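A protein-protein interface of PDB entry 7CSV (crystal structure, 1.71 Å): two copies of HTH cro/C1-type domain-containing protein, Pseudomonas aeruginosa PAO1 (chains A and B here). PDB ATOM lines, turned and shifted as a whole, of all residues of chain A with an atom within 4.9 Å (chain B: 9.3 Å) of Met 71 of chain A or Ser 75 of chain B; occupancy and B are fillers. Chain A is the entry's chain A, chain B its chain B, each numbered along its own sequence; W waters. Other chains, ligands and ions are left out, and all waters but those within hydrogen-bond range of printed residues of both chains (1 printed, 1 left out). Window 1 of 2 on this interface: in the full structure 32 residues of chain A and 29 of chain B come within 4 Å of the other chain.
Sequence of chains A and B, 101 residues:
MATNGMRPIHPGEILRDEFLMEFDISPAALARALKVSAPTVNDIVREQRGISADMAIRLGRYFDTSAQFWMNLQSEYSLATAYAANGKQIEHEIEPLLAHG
The side-chain amide oxygen (OE1) of Gln 68 of chain A is in hydrogen-bond range of the side-chain hydroxyl (OG) of Ser 75 of chain B, at 2.8 Å.
NE2 of Gln 68 of chain A lies within hydrogen-bond range of OE2 of Glu 76 of chain B (2.8 Å).
The side-chain amide oxygen (OD1) of Asn 72 of chain A lies close to the side-chain amide oxygen (OD1) of Asn 72 of chain B, 3.2 Å away.
The side-chain hydroxyl (OG) of Ser 75 of chain A lies within hydrogen-bond range of the side-chain amide oxygen (OE1) of Gln 68 of chain B (2.8 Å).
O of Gln 68 of chain A sits close to ND2 of Asn 72 of chain A, 3.3 Å away.
The side-chain amide nitrogen (ND2) of Asn 72 of chain B sits close to the backbone carbonyl oxygen (O) of Gln 68 of chain B, at 3.3 Å.
OG of Ser 75 of chain B sits at hydrogen-bond distance from O of Met 71 of chain B, 3.4 Å away.
The side-chain hydroxyl (OG) of Ser 75 of chain B is in hydrogen-bond range of the backbone carbonyl oxygen (O) of Asn 72 of chain B, at 3.1 Å.
OG of Ser 78 of chain B is in hydrogen-bond range of NE2 of Gln 74 of chain B (3.1 Å).
Among the printed residues, pairs that only touch across the chains: Ala 53 of chain A with Ser 78 of chain B (3.6 Å), Ala 53 of chain A with Leu 79 of chain B (3.8 Å), Ala 53 of chain A with Ala 82 of chain B (3.8 Å), Ala 67 of chain A with Leu 79 of chain B (3.2 Å), Gln 68 of chain A with Asn 72 of chain B (3.96 Å), Gln 68 of chain A with Leu 79 of chain B (3.8 Å), Met 71 of chain A with Ser 75 of chain B (3.7 Å), Met 71 of chain A with Leu 79 of chain B (3.1 Å), Asn 72 of chain A with Gln 68 of chain B (3.97 Å) and Ser 75 of chain A with Met 71 of chain B (3.8 Å).
Met 71 of chain A touches just these residues of chain B: Ser 75 (3.7 Å) and Leu 79 (3.1 Å).
Of the printed residues of chain A, Ser 75 of chain B touches Gln 68 and Met 71.
Ala 53 of chain A touches just these residues of chain B: Ser 78, Leu 79 and Ala 82.
Of the printed residues of chain A, Asn 72 of chain B touches Gln 68 (3.96 Å) and Asn 72 (3.2 Å).
Printed residues of chain A within 4 Å of Glu 76 of chain B: Gln 68 (2.8 Å).
Of the printed residues of chain B, Ser 75 of chain A touches Gln 68 and Met 71.
Of the printed residues of chain B, Asn 72 of chain A touches Gln 68 (3.97 Å) and Asn 72 (3.2 Å).
Trp 70 of chain B touches none of the printed residues of chain A.
Ser 52 of chain A touches none of the printed residues of chain B.
The nearest residue of chain A that does not touch Ser 75 of chain B is Asn 72 of chain A (4.2 Å).
Hydrophobic or aromatic side chains of chain A within 4 Å of the printed part of chain B: Ala 53, Ala 67 and Met 71.
Printed residues of chain B that touch a printed residue of chain A: Gln 68, Met 71, Asn 72, Ser 75, Glu 76, Ser 78, Leu 79 and Ala 82.
Hydrophobic or aromatic side chains of chain B that line the printed part of chain A: Met 71, Leu 79 and Ala 82.
Among the printed residues, 14 pairs touch across the chains.
Gln 68 of chain A touches Asn 72 of chain B, and with the chains exchanged Asn 72 of chain A touches Gln 68 of chain B.
Gln 68 of chain A touches Ser 75 of chain B, and with the chains exchanged Ser 75 of chain A touches Gln 68 of chain B.
Met 71 of chain A touches Ser 75 of chain B, and with the chains exchanged Ser 75 of chain A touches Met 71 of chain B.
Asn 72 of chain A touches its own counterpart, Asn 72 of chain B.
Water W1 bridges the backbone carbonyl oxygen of Asn 72 of chain A and the side-chain amide nitrogen of Gln 68 of chain B.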
ATOM      1  N   ILE A  51       8.382 -24.326   8.638  1.00  0.00           N
ATOM      2  CA  ILE A  51       7.153 -23.760   9.194  1.00  0.00           C
ATOM      3  C   ILE A  51       7.516 -22.564  10.058  1.00  0.00           C
ATOM      4  O   ILE A  51       8.207 -22.708  11.074  1.00  0.00           O
ATOM      5  CB  ILE A  51       6.393 -24.796  10.033  1.00  0.00           C
ATOM      6  CG1 ILE A  51       6.192 -26.094   9.264  1.00  0.00           C
ATOM      7  CG2 ILE A  51       5.054 -24.223  10.510  1.00  0.00           C
ATOM      8  CD1 ILE A  51       5.401 -25.921   8.060  1.00  0.00           C
ATOM      9  N   SER A  52       7.035 -21.389   9.670  1.00  0.00           N
ATOM     10  CA  SER A  52       7.154 -20.205  10.500  1.00  0.00           C
ATOM     11  C   SER A  52       6.087 -20.210  11.596  1.00  0.00           C
ATOM     12  O   SER A  52       5.091 -20.936  11.535  1.00  0.00           O
ATOM     13  CB  SER A  52       6.995 -18.943   9.656  1.00  0.00           C
ATOM     14  OG  SER A  52       5.642 -18.821   9.218  1.00  0.00           O
ATOM     15  N   ALA A  53       6.294 -19.353  12.600  1.00  0.00           N
ATOM     16  CA  ALA A  53       5.299 -19.222  13.662  1.00  0.00           C
ATOM     17  C   ALA A  53       3.943 -18.848  13.092  1.00  0.00           C
ATOM     18  O   ALA A  53       2.922 -19.413  13.491  1.00  0.00           O
ATOM     19  CB  ALA A  53       5.746 -18.182  14.685  1.00  0.00           C
ATOM     20  N   ALA A  56       2.431 -21.809  11.496  1.00  0.00           N
ATOM     21  CA  ALA A  56       1.991 -22.796  12.480  1.00  0.00           C
ATOM     22  C   ALA A  56       0.643 -22.427  13.063  1.00  0.00           C
ATOM     23  O   ALA A  56      -0.192 -23.302  13.331  1.00  0.00           O
ATOM     24  CB  ALA A  56       3.015 -22.914  13.607  1.00  0.00           C
ATOM     25  N   ALA A  67      -0.790 -24.836  17.550  1.00  0.00           N
ATOM     26  CA  ALA A  67       0.291 -24.317  16.725  1.00  0.00           C
ATOM     27  C   ALA A  67       1.618 -24.954  17.108  1.00  0.00           C
ATOM     28  O   ALA A  67       2.478 -25.158  16.247  1.00  0.00           O
ATOM     29  CB  ALA A  67       0.367 -22.797  16.849  1.00  0.00           C
ATOM     30  N   GLN A  68       1.774 -25.312  18.385  1.00  0.00           N
ATOM     31  CA  GLN A  68       3.007 -25.940  18.848  1.00  0.00           C
ATOM     32  C   GLN A  68       3.242 -27.291  18.195  1.00  0.00           C
ATOM     33  O   GLN A  68       4.396 -27.700  18.040  1.00  0.00           O
ATOM     34  CB  GLN A  68       2.979 -26.084  20.366  1.00  0.00           C
ATOM     35  CG  GLN A  68       3.304 -24.792  21.089  1.00  0.00           C
ATOM     36  CD  GLN A  68       4.803 -24.547  21.236  1.00  0.00           C
ATOM     37  OE1 GLN A  68       5.622 -25.008  20.427  1.00  0.00           O
ATOM     38  NE2 GLN A  68       5.166 -23.824  22.272  1.00  0.00           N
ATOM     39  N   PHE A  69       2.172 -28.015  17.853  1.00  0.00           N
ATOM     40  CA  PHE A  69       2.328 -29.277  17.133  1.00  0.00           C
ATOM     41  C   PHE A  69       3.231 -29.091  15.921  1.00  0.00           C
ATOM     42  O   PHE A  69       4.193 -29.843  15.724  1.00  0.00           O
ATOM     43  CB  PHE A  69       0.955 -29.815  16.706  1.00  0.00           C
ATOM     44  CG  PHE A  69       1.021 -30.998  15.758  1.00  0.00           C
ATOM     45  CD1 PHE A  69       1.246 -32.288  16.238  1.00  0.00           C
ATOM     46  CD2 PHE A  69       0.850 -30.817  14.394  1.00  0.00           C
ATOM     47  CE1 PHE A  69       1.297 -33.376  15.360  1.00  0.00           C
ATOM     48  CE2 PHE A  69       0.893 -31.894  13.509  1.00  0.00           C
ATOM     49  CZ  PHE A  69       1.114 -33.175  13.994  1.00  0.00           C
ATOM     50  N   TRP A  70       2.952 -28.056  15.121  1.00  0.00           N
ATOM     51  CA  TRP A  70       3.745 -27.799  13.925  1.00  0.00           C
ATOM     52  C   TRP A  70       5.121 -27.262  14.270  1.00  0.00           C
ATOM     53  O   TRP A  70       6.101 -27.615  13.612  1.00  0.00           O
ATOM     54  CB  TRP A  70       3.008 -26.825  13.012  1.00  0.00           C
ATOM     55  CG  TRP A  70       1.741 -27.425  12.555  1.00  0.00           C
ATOM     56  CD1 TRP A  70       0.504 -27.214  13.076  1.00  0.00           C
ATOM     57  CD2 TRP A  70       1.590 -28.401  11.529  1.00  0.00           C
ATOM     58  NE1 TRP A  70      -0.422 -27.975  12.412  1.00  0.00           N
ATOM     59  CE2 TRP A  70       0.214 -28.716  11.456  1.00  0.00           C
ATOM     60  CE3 TRP A  70       2.477 -29.024  10.648  1.00  0.00           C
ATOM     61  CZ2 TRP A  70      -0.298 -29.634  10.537  1.00  0.00           C
ATOM     62  CZ3 TRP A  70       1.969 -29.941   9.736  1.00  0.00           C
ATOM     63  CH2 TRP A  70       0.594 -30.230   9.685  1.00  0.00           C
ATOM     64  N   MET A  71       5.215 -26.398  15.282  1.00  0.00           N
ATOM     65  CA  MET A  71       6.522 -25.859  15.631  1.00  0.00           C
ATOM     66  C   MET A  71       7.402 -26.938  16.228  1.00  0.00           C
ATOM     67  O   MET A  71       8.626 -26.878  16.080  1.00  0.00           O
ATOM     68  CB  MET A  71       6.399 -24.701  16.609  1.00  0.00           C
ATOM     69  CG  MET A  71       5.736 -23.478  15.991  1.00  0.00           C
ATOM     70  SD  MET A  71       6.586 -22.756  14.583  1.00  0.00           S
ATOM     71  CE  MET A  71       7.886 -21.855  15.436  1.00  0.00           C
ATOM     72  N   ASN A  72       6.799 -27.917  16.909  1.00  0.00           N
ATOM     73  CA  ASN A  72       7.587 -29.022  17.455  1.00  0.00           C
ATOM     74  C   ASN A  72       8.141 -29.895  16.337  1.00  0.00           C
ATOM     75  O   ASN A  72       9.282 -30.367  16.416  1.00  0.00           O
ATOM     76  CB  ASN A  72       6.738 -29.858  18.422  1.00  0.00           C
ATOM     77  CG  ASN A  72       6.440 -29.139  19.740  1.00  0.00           C
ATOM     78  OD1 ASN A  72       7.098 -28.152  20.100  1.00  0.00           O
ATOM     79  ND2 ASN A  72       5.447 -29.645  20.470  1.00  0.00           N
ATOM     80  N   LEU A  73       7.352 -30.121  15.277  1.00  0.00           N
ATOM     81  CA  LEU A  73       7.882 -30.852  14.128  1.00  0.00           C
ATOM     82  C   LEU A  73       9.015 -30.076  13.477  1.00  0.00           C
ATOM     83  O   LEU A  73      10.036 -30.653  13.077  1.00  0.00           O
ATOM     84  CB  LEU A  73       6.778 -31.111  13.107  1.00  0.00           C
ATOM     85  CG  LEU A  73       5.625 -32.007  13.555  1.00  0.00           C
ATOM     86  CD1 LEU A  73       4.567 -32.073  12.461  1.00  0.00           C
ATOM     87  CD2 LEU A  73       6.152 -33.396  13.901  1.00  0.00           C
ATOM     88  N   GLN A  74       8.856 -28.757  13.380  1.00  0.00           N
ATOM     89  CA  GLN A  74       9.894 -27.925  12.788  1.00  0.00           C
ATOM     90  C   GLN A  74      11.164 -27.955  13.624  1.00  0.00           C
ATOM     91  O   GLN A  74      12.271 -28.078  13.082  1.00  0.00           O
ATOM     92  CB  GLN A  74       9.383 -26.490  12.638  1.00  0.00           C
ATOM     93  CG  GLN A  74      10.440 -25.539  12.072  1.00  0.00           C
ATOM     94  CD  GLN A  74      10.843 -25.904  10.671  1.00  0.00           C
ATOM     95  OE1 GLN A  74      10.007 -26.284   9.849  1.00  0.00           O
ATOM     96  NE2 GLN A  74      12.141 -25.812  10.383  1.00  0.00           N
ATOM     97  N   SER A  75      11.031 -27.832  14.943  1.00  0.00           N
ATOM     98  CA  SER A  75      12.222 -27.829  15.782  1.00  0.00           C
ATOM     99  C   SER A  75      12.950 -29.162  15.695  1.00  0.00           C
ATOM    100  O   SER A  75      14.190 -29.202  15.673  1.00  0.00           O
ATOM    101  CB  SER A  75      11.853 -27.515  17.225  1.00  0.00           C
ATOM    102  OG  SER A  75      11.046 -28.524  17.773  1.00  0.00           O
ATOM    103  N   GLY B   5      -2.507 -18.258  22.955  1.00  0.00           N
ATOM    104  CA  GLY B   5      -1.387 -17.977  23.831  1.00  0.00           C
ATOM    105  C   GLY B   5      -0.686 -16.684  23.480  1.00  0.00           C
ATOM    106  O   GLY B   5      -0.087 -16.565  22.408  1.00  0.00           O
ATOM    107  N   PRO B   8       4.346 -13.610  26.224  1.00  0.00           N
ATOM    108  CA  PRO B   8       5.624 -14.217  25.835  1.00  0.00           C
ATOM    109  C   PRO B   8       6.583 -14.302  27.016  1.00  0.00           C
ATOM    110  O   PRO B   8       6.738 -13.349  27.783  1.00  0.00           O
ATOM    111  CB  PRO B   8       6.157 -13.275  24.747  1.00  0.00           C
ATOM    112  CG  PRO B   8       5.064 -12.302  24.470  1.00  0.00           C
ATOM    113  CD  PRO B   8       4.225 -12.240  25.713  1.00  0.00           C
ATOM    114  N   ILE B   9       7.216 -15.462  27.158  1.00  0.00           N
ATOM    115  CA  ILE B   9       8.313 -15.673  28.096  1.00  0.00           C
ATOM    116  C   ILE B   9       9.535 -15.976  27.252  1.00  0.00           C
ATOM    117  O   ILE B   9       9.618 -17.048  26.647  1.00  0.00           O
ATOM    118  CB  ILE B   9       8.040 -16.823  29.066  1.00  0.00           C
ATOM    119  CG1 ILE B   9       6.699 -16.641  29.753  1.00  0.00           C
ATOM    120  CG2 ILE B   9       9.174 -16.940  30.084  1.00  0.00           C
ATOM    121  CD1 ILE B   9       6.103 -17.955  30.138  1.00  0.00           C
ATOM    122  N   HIS B  10      10.470 -15.042  27.197  1.00  0.00           N
ATOM    123  CA  HIS B  10      11.624 -15.243  26.344  1.00  0.00           C
ATOM    124  C   HIS B  10      12.499 -16.348  26.933  1.00  0.00           C
ATOM    125  O   HIS B  10      12.673 -16.410  28.155  1.00  0.00           O
ATOM    126  CB  HIS B  10      12.416 -13.940  26.201  1.00  0.00           C
ATOM    127  CG  HIS B  10      13.410 -13.960  25.082  1.00  0.00           C
ATOM    128  ND1 HIS B  10      14.655 -14.533  25.210  1.00  0.00           N
ATOM    129  CD2 HIS B  10      13.347 -13.473  23.821  1.00  0.00           C
ATOM    130  CE1 HIS B  10      15.315 -14.407  24.072  1.00  0.00           C
ATOM    131  NE2 HIS B  10      14.540 -13.772  23.210  1.00  0.00           N
ATOM    132  N   PRO B  11      13.008 -17.266  26.102  1.00  0.00           N
ATOM    133  CA  PRO B  11      13.904 -18.320  26.611  1.00  0.00           C
ATOM    134  C   PRO B  11      15.056 -17.786  27.437  1.00  0.00           C
ATOM    135  O   PRO B  11      15.533 -18.486  28.343  1.00  0.00           O
ATOM    136  CB  PRO B  11      14.410 -19.002  25.333  1.00  0.00           C
ATOM    137  CG  PRO B  11      13.373 -18.706  24.306  1.00  0.00           C
ATOM    138  CD  PRO B  11      12.796 -17.370  24.649  1.00  0.00           C
ATOM    139  N   GLY B  50      16.787 -14.870  19.600  1.00  0.00           N
ATOM    140  CA  GLY B  50      16.297 -16.181  19.972  1.00  0.00           C
ATOM    141  C   GLY B  50      17.375 -17.252  19.974  1.00  0.00           C
ATOM    142  O   GLY B  50      18.529 -17.039  19.596  1.00  0.00           O
ATOM    143  N   ILE B  51      16.971 -18.438  20.422  1.00  0.00           N
ATOM    144  CA  ILE B  51      17.853 -19.598  20.477  1.00  0.00           C
ATOM    145  C   ILE B  51      17.786 -20.344  19.146  1.00  0.00           C
ATOM    146  O   ILE B  51      16.714 -20.793  18.721  1.00  0.00           O
ATOM    147  CB  ILE B  51      17.475 -20.512  21.651  1.00  0.00           C
ATOM    148  CG1 ILE B  51      17.806 -19.820  22.978  1.00  0.00           C
ATOM    149  CG2 ILE B  51      18.241 -21.814  21.571  1.00  0.00           C
ATOM    150  CD1 ILE B  51      17.377 -20.599  24.217  1.00  0.00           C
ATOM    151  N   SER B  52      18.932 -20.473  18.477  1.00  0.00           N
ATOM    152  CA  SER B  52      19.025 -21.254  17.252  1.00  0.00           C
ATOM    153  C   SER B  52      19.145 -22.742  17.572  1.00  0.00           C
ATOM    154  O   SER B  52      19.433 -23.138  18.705  1.00  0.00           O
ATOM    155  CB  SER B  52      20.237 -20.829  16.426  1.00  0.00           C
ATOM    156  OG  SER B  52      21.440 -21.227  17.073  1.00  0.00           O
ATOM    157  N   ALA B  67      18.123 -30.814  23.833  1.00  0.00           N
ATOM    158  CA  ALA B  67      18.064 -29.607  23.008  1.00  0.00           C
ATOM    159  C   ALA B  67      16.623 -29.150  22.795  1.00  0.00           C
ATOM    160  O   ALA B  67      16.361 -27.943  22.713  1.00  0.00           O
ATOM    161  CB  ALA B  67      18.753 -29.840  21.662  1.00  0.00           C
ATOM    162  N   GLN B  68      15.684 -30.092  22.710  1.00  0.00           N
ATOM    163  CA  GLN B  68      14.289 -29.715  22.504  1.00  0.00           C
ATOM    164  C   GLN B  68      13.750 -28.885  23.660  1.00  0.00           C
ATOM    165  O   GLN B  68      12.834 -28.087  23.458  1.00  0.00           O
ATOM    166  CB  GLN B  68      13.414 -30.956  22.277  1.00  0.00           C
ATOM    167  CG  GLN B  68      13.490 -31.537  20.852  1.00  0.00           C
ATOM    168  CD  GLN B  68      12.674 -30.764  19.800  1.00  0.00           C
ATOM    169  OE1 GLN B  68      12.323 -29.593  19.984  1.00  0.00           O
ATOM    170  NE2 GLN B  68      12.371 -31.430  18.680  1.00  0.00           N
ATOM    171  N   PHE B  69      14.293 -29.034  24.871  1.00  0.00           N
ATOM    172  CA  PHE B  69      13.841 -28.173  25.967  1.00  0.00           C
ATOM    173  C   PHE B  69      13.976 -26.705  25.586  1.00  0.00           C
ATOM    174  O   PHE B  69      13.048 -25.909  25.779  1.00  0.00           O
ATOM    175  CB  PHE B  69      14.636 -28.484  27.243  1.00  0.00           C
ATOM    176  CG  PHE B  69      14.427 -27.500  28.368  1.00  0.00           C
ATOM    177  CD1 PHE B  69      13.337 -27.616  29.221  1.00  0.00           C
ATOM    178  CD2 PHE B  69      15.347 -26.476  28.597  1.00  0.00           C
ATOM    179  CE1 PHE B  69      13.150 -26.710  30.272  1.00  0.00           C
ATOM    180  CE2 PHE B  69      15.173 -25.568  29.649  1.00  0.00           C
ATOM    181  CZ  PHE B  69      14.063 -25.684  30.485  1.00  0.00           C
ATOM    182  N   TRP B  70      15.117 -26.338  25.007  1.00  0.00           N
ATOM    183  CA  TRP B  70      15.374 -24.958  24.623  1.00  0.00           C
ATOM    184  C   TRP B  70      14.588 -24.572  23.381  1.00  0.00           C
ATOM    185  O   TRP B  70      14.061 -23.458  23.297  1.00  0.00           O
ATOM    186  CB  TRP B  70      16.878 -24.769  24.416  1.00  0.00           C
ATOM    187  CG  TRP B  70      17.608 -25.027  25.701  1.00  0.00           C
ATOM    188  CD1 TRP B  70      18.327 -26.148  26.053  1.00  0.00           C
ATOM    189  CD2 TRP B  70      17.645 -24.156  26.824  1.00  0.00           C
ATOM    190  NE1 TRP B  70      18.809 -26.006  27.334  1.00  0.00           N
ATOM    191  CE2 TRP B  70      18.412 -24.787  27.824  1.00  0.00           C
ATOM    192  CE3 TRP B  70      17.118 -22.887  27.075  1.00  0.00           C
ATOM    193  CZ2 TRP B  70      18.663 -24.188  29.057  1.00  0.00           C
ATOM    194  CZ3 TRP B  70      17.348 -22.303  28.303  1.00  0.00           C
ATOM    195  CH2 TRP B  70      18.114 -22.949  29.279  1.00  0.00           C
ATOM    196  N   MET B  71      14.478 -25.486  22.419  1.00  0.00           N
ATOM    197  CA  MET B  71      13.729 -25.168  21.216  1.00  0.00           C
ATOM    198  C   MET B  71      12.248 -25.038  21.518  1.00  0.00           C
ATOM    199  O   MET B  71      11.559 -24.238  20.873  1.00  0.00           O
ATOM    200  CB  MET B  71      13.959 -26.236  20.146  1.00  0.00           C
ATOM    201  CG  MET B  71      15.390 -26.302  19.685  1.00  0.00           C
ATOM    202  SD  MET B  71      15.869 -24.819  18.783  1.00  0.00           S
ATOM    203  CE  MET B  71      15.122 -25.188  17.195  1.00  0.00           C
ATOM    204  N   ASN B  72      11.745 -25.807  22.490  1.00  0.00           N
ATOM    205  CA  ASN B  72      10.336 -25.693  22.858  1.00  0.00           C
ATOM    206  C   ASN B  72      10.049 -24.355  23.534  1.00  0.00           C
ATOM    207  O   ASN B  72       8.984 -23.760  23.316  1.00  0.00           O
ATOM    208  CB  ASN B  72       9.927 -26.851  23.778  1.00  0.00           C
ATOM    209  CG  ASN B  72       9.826 -28.196  23.054  1.00  0.00           C
ATOM    210  OD1 ASN B  72       9.776 -28.274  21.815  1.00  0.00           O
ATOM    211  ND2 ASN B  72       9.772 -29.271  23.839  1.00  0.00           N
ATOM    212  N   LEU B  73      10.981 -23.861  24.356  1.00  0.00           N
ATOM    213  CA  LEU B  73      10.800 -22.520  24.917  1.00  0.00           C
ATOM    214  C   LEU B  73      10.831 -21.469  23.817  1.00  0.00           C
ATOM    215  O   LEU B  73      10.056 -20.506  23.842  1.00  0.00           O
ATOM    216  CB  LEU B  73      11.883 -22.215  25.955  1.00  0.00           C
ATOM    217  CG  LEU B  73      11.880 -23.021  27.259  1.00  0.00           C
ATOM    218  CD1 LEU B  73      13.077 -22.619  28.104  1.00  0.00           C
ATOM    219  CD2 LEU B  73      10.573 -22.784  27.992  1.00  0.00           C
ATOM    220  N   GLN B  74      11.734 -21.630  22.847  1.00  0.00           N
ATOM    221  CA  GLN B  74      11.822 -20.666  21.752  1.00  0.00           C
ATOM    222  C   GLN B  74      10.547 -20.647  20.921  1.00  0.00           C
ATOM    223  O   GLN B  74      10.045 -19.578  20.571  1.00  0.00           O
ATOM    224  CB  GLN B  74      13.025 -20.968  20.863  1.00  0.00           C
ATOM    225  CG  GLN B  74      13.170 -19.994  19.694  1.00  0.00           C
ATOM    226  CD  GLN B  74      13.332 -18.560  20.155  1.00  0.00           C
ATOM    227  OE1 GLN B  74      14.159 -18.269  21.008  1.00  0.00           O
ATOM    228  NE2 GLN B  74      12.511 -17.652  19.612  1.00  0.00           N
ATOM    229  N   SER B  75      10.012 -21.820  20.577  1.00  0.00           N
ATOM    230  CA  SER B  75       8.802 -21.838  19.759  1.00  0.00           C
ATOM    231  C   SER B  75       7.607 -21.254  20.509  1.00  0.00           C
ATOM    232  O   SER B  75       6.759 -20.590  19.903  1.00  0.00           O
ATOM    233  CB  SER B  75       8.495 -23.255  19.283  1.00  0.00           C
ATOM    234  OG  SER B  75       8.230 -24.115  20.359  1.00  0.00           O
ATOM    235  N   GLU B  76       7.504 -21.510  21.820  1.00  0.00           N
ATOM    236  CA  GLU B  76       6.439 -20.874  22.592  1.00  0.00           C
ATOM    237  C   GLU B  76       6.553 -19.359  22.517  1.00  0.00           C
ATOM    238  O   GLU B  76       5.551 -18.664  22.330  1.00  0.00           O
ATOM    239  CB  GLU B  76       6.464 -21.347  24.052  1.00  0.00           C
ATOM    240  CG  GLU B  76       5.449 -20.631  24.971  1.00  0.00           C
ATOM    241  CD  GLU B  76       4.023 -21.151  24.817  1.00  0.00           C
ATOM    242  OE1 GLU B  76       3.092 -20.538  25.403  1.00  0.00           O
ATOM    243  OE2 GLU B  76       3.819 -22.164  24.108  1.00  0.00           O
ATOM    244  N   TYR B  77       7.775 -18.829  22.621  1.00  0.00           N
ATOM    245  CA  TYR B  77       7.949 -17.378  22.541  1.00  0.00           C
ATOM    246  C   TYR B  77       7.612 -16.867  21.145  1.00  0.00           C
ATOM    247  O   TYR B  77       6.920 -15.850  20.991  1.00  0.00           O
ATOM    248  CB  TYR B  77       9.381 -16.986  22.915  1.00  0.00           C
ATOM    249  CG  TYR B  77       9.627 -15.500  22.735  1.00  0.00           C
ATOM    250  CD1 TYR B  77       9.264 -14.593  23.724  1.00  0.00           C
ATOM    251  CD2 TYR B  77      10.204 -15.007  21.566  1.00  0.00           C
ATOM    252  CE1 TYR B  77       9.479 -13.235  23.565  1.00  0.00           C
ATOM    253  CE2 TYR B  77      10.431 -13.650  21.395  1.00  0.00           C
ATOM    254  CZ  TYR B  77      10.061 -12.771  22.398  1.00  0.00           C
ATOM    255  OH  TYR B  77      10.274 -11.414  22.233  1.00  0.00           O
ATOM    256  N   SER B  78       8.111 -17.555  20.112  1.00  0.00           N
ATOM    257  CA  SER B  78       7.814 -17.156  18.735  1.00  0.00           C
ATOM    258  C   SER B  78       6.322 -17.217  18.458  1.00  0.00           C
ATOM    259  O   SER B  78       5.769 -16.331  17.789  1.00  0.00           O
ATOM    260  CB  SER B  78       8.555 -18.044  17.743  1.00  0.00           C
ATOM    261  OG  SER B  78       9.957 -17.849  17.833  1.00  0.00           O
ATOM    262  N   LEU B  79       5.651 -18.261  18.953  1.00  0.00           N
ATOM    263  CA  LEU B  79       4.203 -18.329  18.773  1.00  0.00           C
ATOM    264  C   LEU B  79       3.507 -17.194  19.504  1.00  0.00           C
ATOM    265  O   LEU B  79       2.576 -16.574  18.967  1.00  0.00           O
ATOM    266  CB  LEU B  79       3.604 -19.647  19.280  1.00  0.00           C
ATOM    267  CG  LEU B  79       3.454 -20.945  18.445  1.00  0.00           C
ATOM    268  CD1 LEU B  79       2.790 -20.713  17.045  1.00  0.00           C
ATOM    269  CD2 LEU B  79       4.610 -21.943  18.452  1.00  0.00           C
ATOM    270  N   ALA B  80       3.905 -16.958  20.761  1.00  0.00           N
ATOM    271  CA  ALA B  80       3.232 -15.931  21.562  1.00  0.00           C
ATOM    272  C   ALA B  80       3.351 -14.557  20.914  1.00  0.00           C
ATOM    273  O   ALA B  80       2.370 -13.799  20.868  1.00  0.00           O
ATOM    274  CB  ALA B  80       3.803 -15.900  22.980  1.00  0.00           C
ATOM    275  N   THR B  81       4.536 -14.211  20.405  1.00  0.00           N
ATOM    276  CA  THR B  81       4.655 -12.897  19.771  1.00  0.00           C
ATOM    277  C   THR B  81       3.898 -12.869  18.444  1.00  0.00           C
ATOM    278  O   THR B  81       3.234 -11.876  18.124  1.00  0.00           O
ATOM    279  CB  THR B  81       6.125 -12.519  19.584  1.00  0.00           C
ATOM    280  OG1 THR B  81       6.777 -13.502  18.768  1.00  0.00           O
ATOM    281  CG2 THR B  81       6.820 -12.464  20.937  1.00  0.00           C
ATOM    282  N   ALA B  82       3.978 -13.952  17.663  1.00  0.00           N
ATOM    283  CA  ALA B  82       3.220 -14.015  16.412  1.00  0.00           C
ATOM    284  C   ALA B  82       1.726 -13.879  16.658  1.00  0.00           C
ATOM    285  O   ALA B  82       1.024 -13.209  15.891  1.00  0.00           O
ATOM    286  CB  ALA B  82       3.499 -15.322  15.668  1.00  0.00           C
ATOM    287  N   TYR B  83       1.216 -14.527  17.705  1.00  0.00           N
ATOM    288  CA  TYR B  83      -0.219 -14.455  17.980  1.00  0.00           C
ATOM    289  C   TYR B  83      -0.623 -13.071  18.478  1.00  0.00           C
ATOM    290  O   TYR B  83      -1.711 -12.561  18.137  1.00  0.00           O
ATOM    291  CB  TYR B  83      -0.604 -15.529  18.996  1.00  0.00           C
ATOM    292  CG  TYR B  83      -2.094 -15.701  19.103  1.00  0.00           C
ATOM    293  CD1 TYR B  83      -2.774 -16.583  18.270  1.00  0.00           C
ATOM    294  CD2 TYR B  83      -2.826 -14.936  19.992  1.00  0.00           C
ATOM    295  CE1 TYR B  83      -4.146 -16.721  18.350  1.00  0.00           C
ATOM    296  CE2 TYR B  83      -4.191 -15.055  20.081  1.00  0.00           C
ATOM    297  CZ  TYR B  83      -4.849 -15.948  19.261  1.00  0.00           C
ATOM    298  OH  TYR B  83      -6.219 -16.062  19.372  1.00  0.00           O
HETATM  299  O   HOH W   1       9.107 -32.567  18.198  1.00  0.00           O
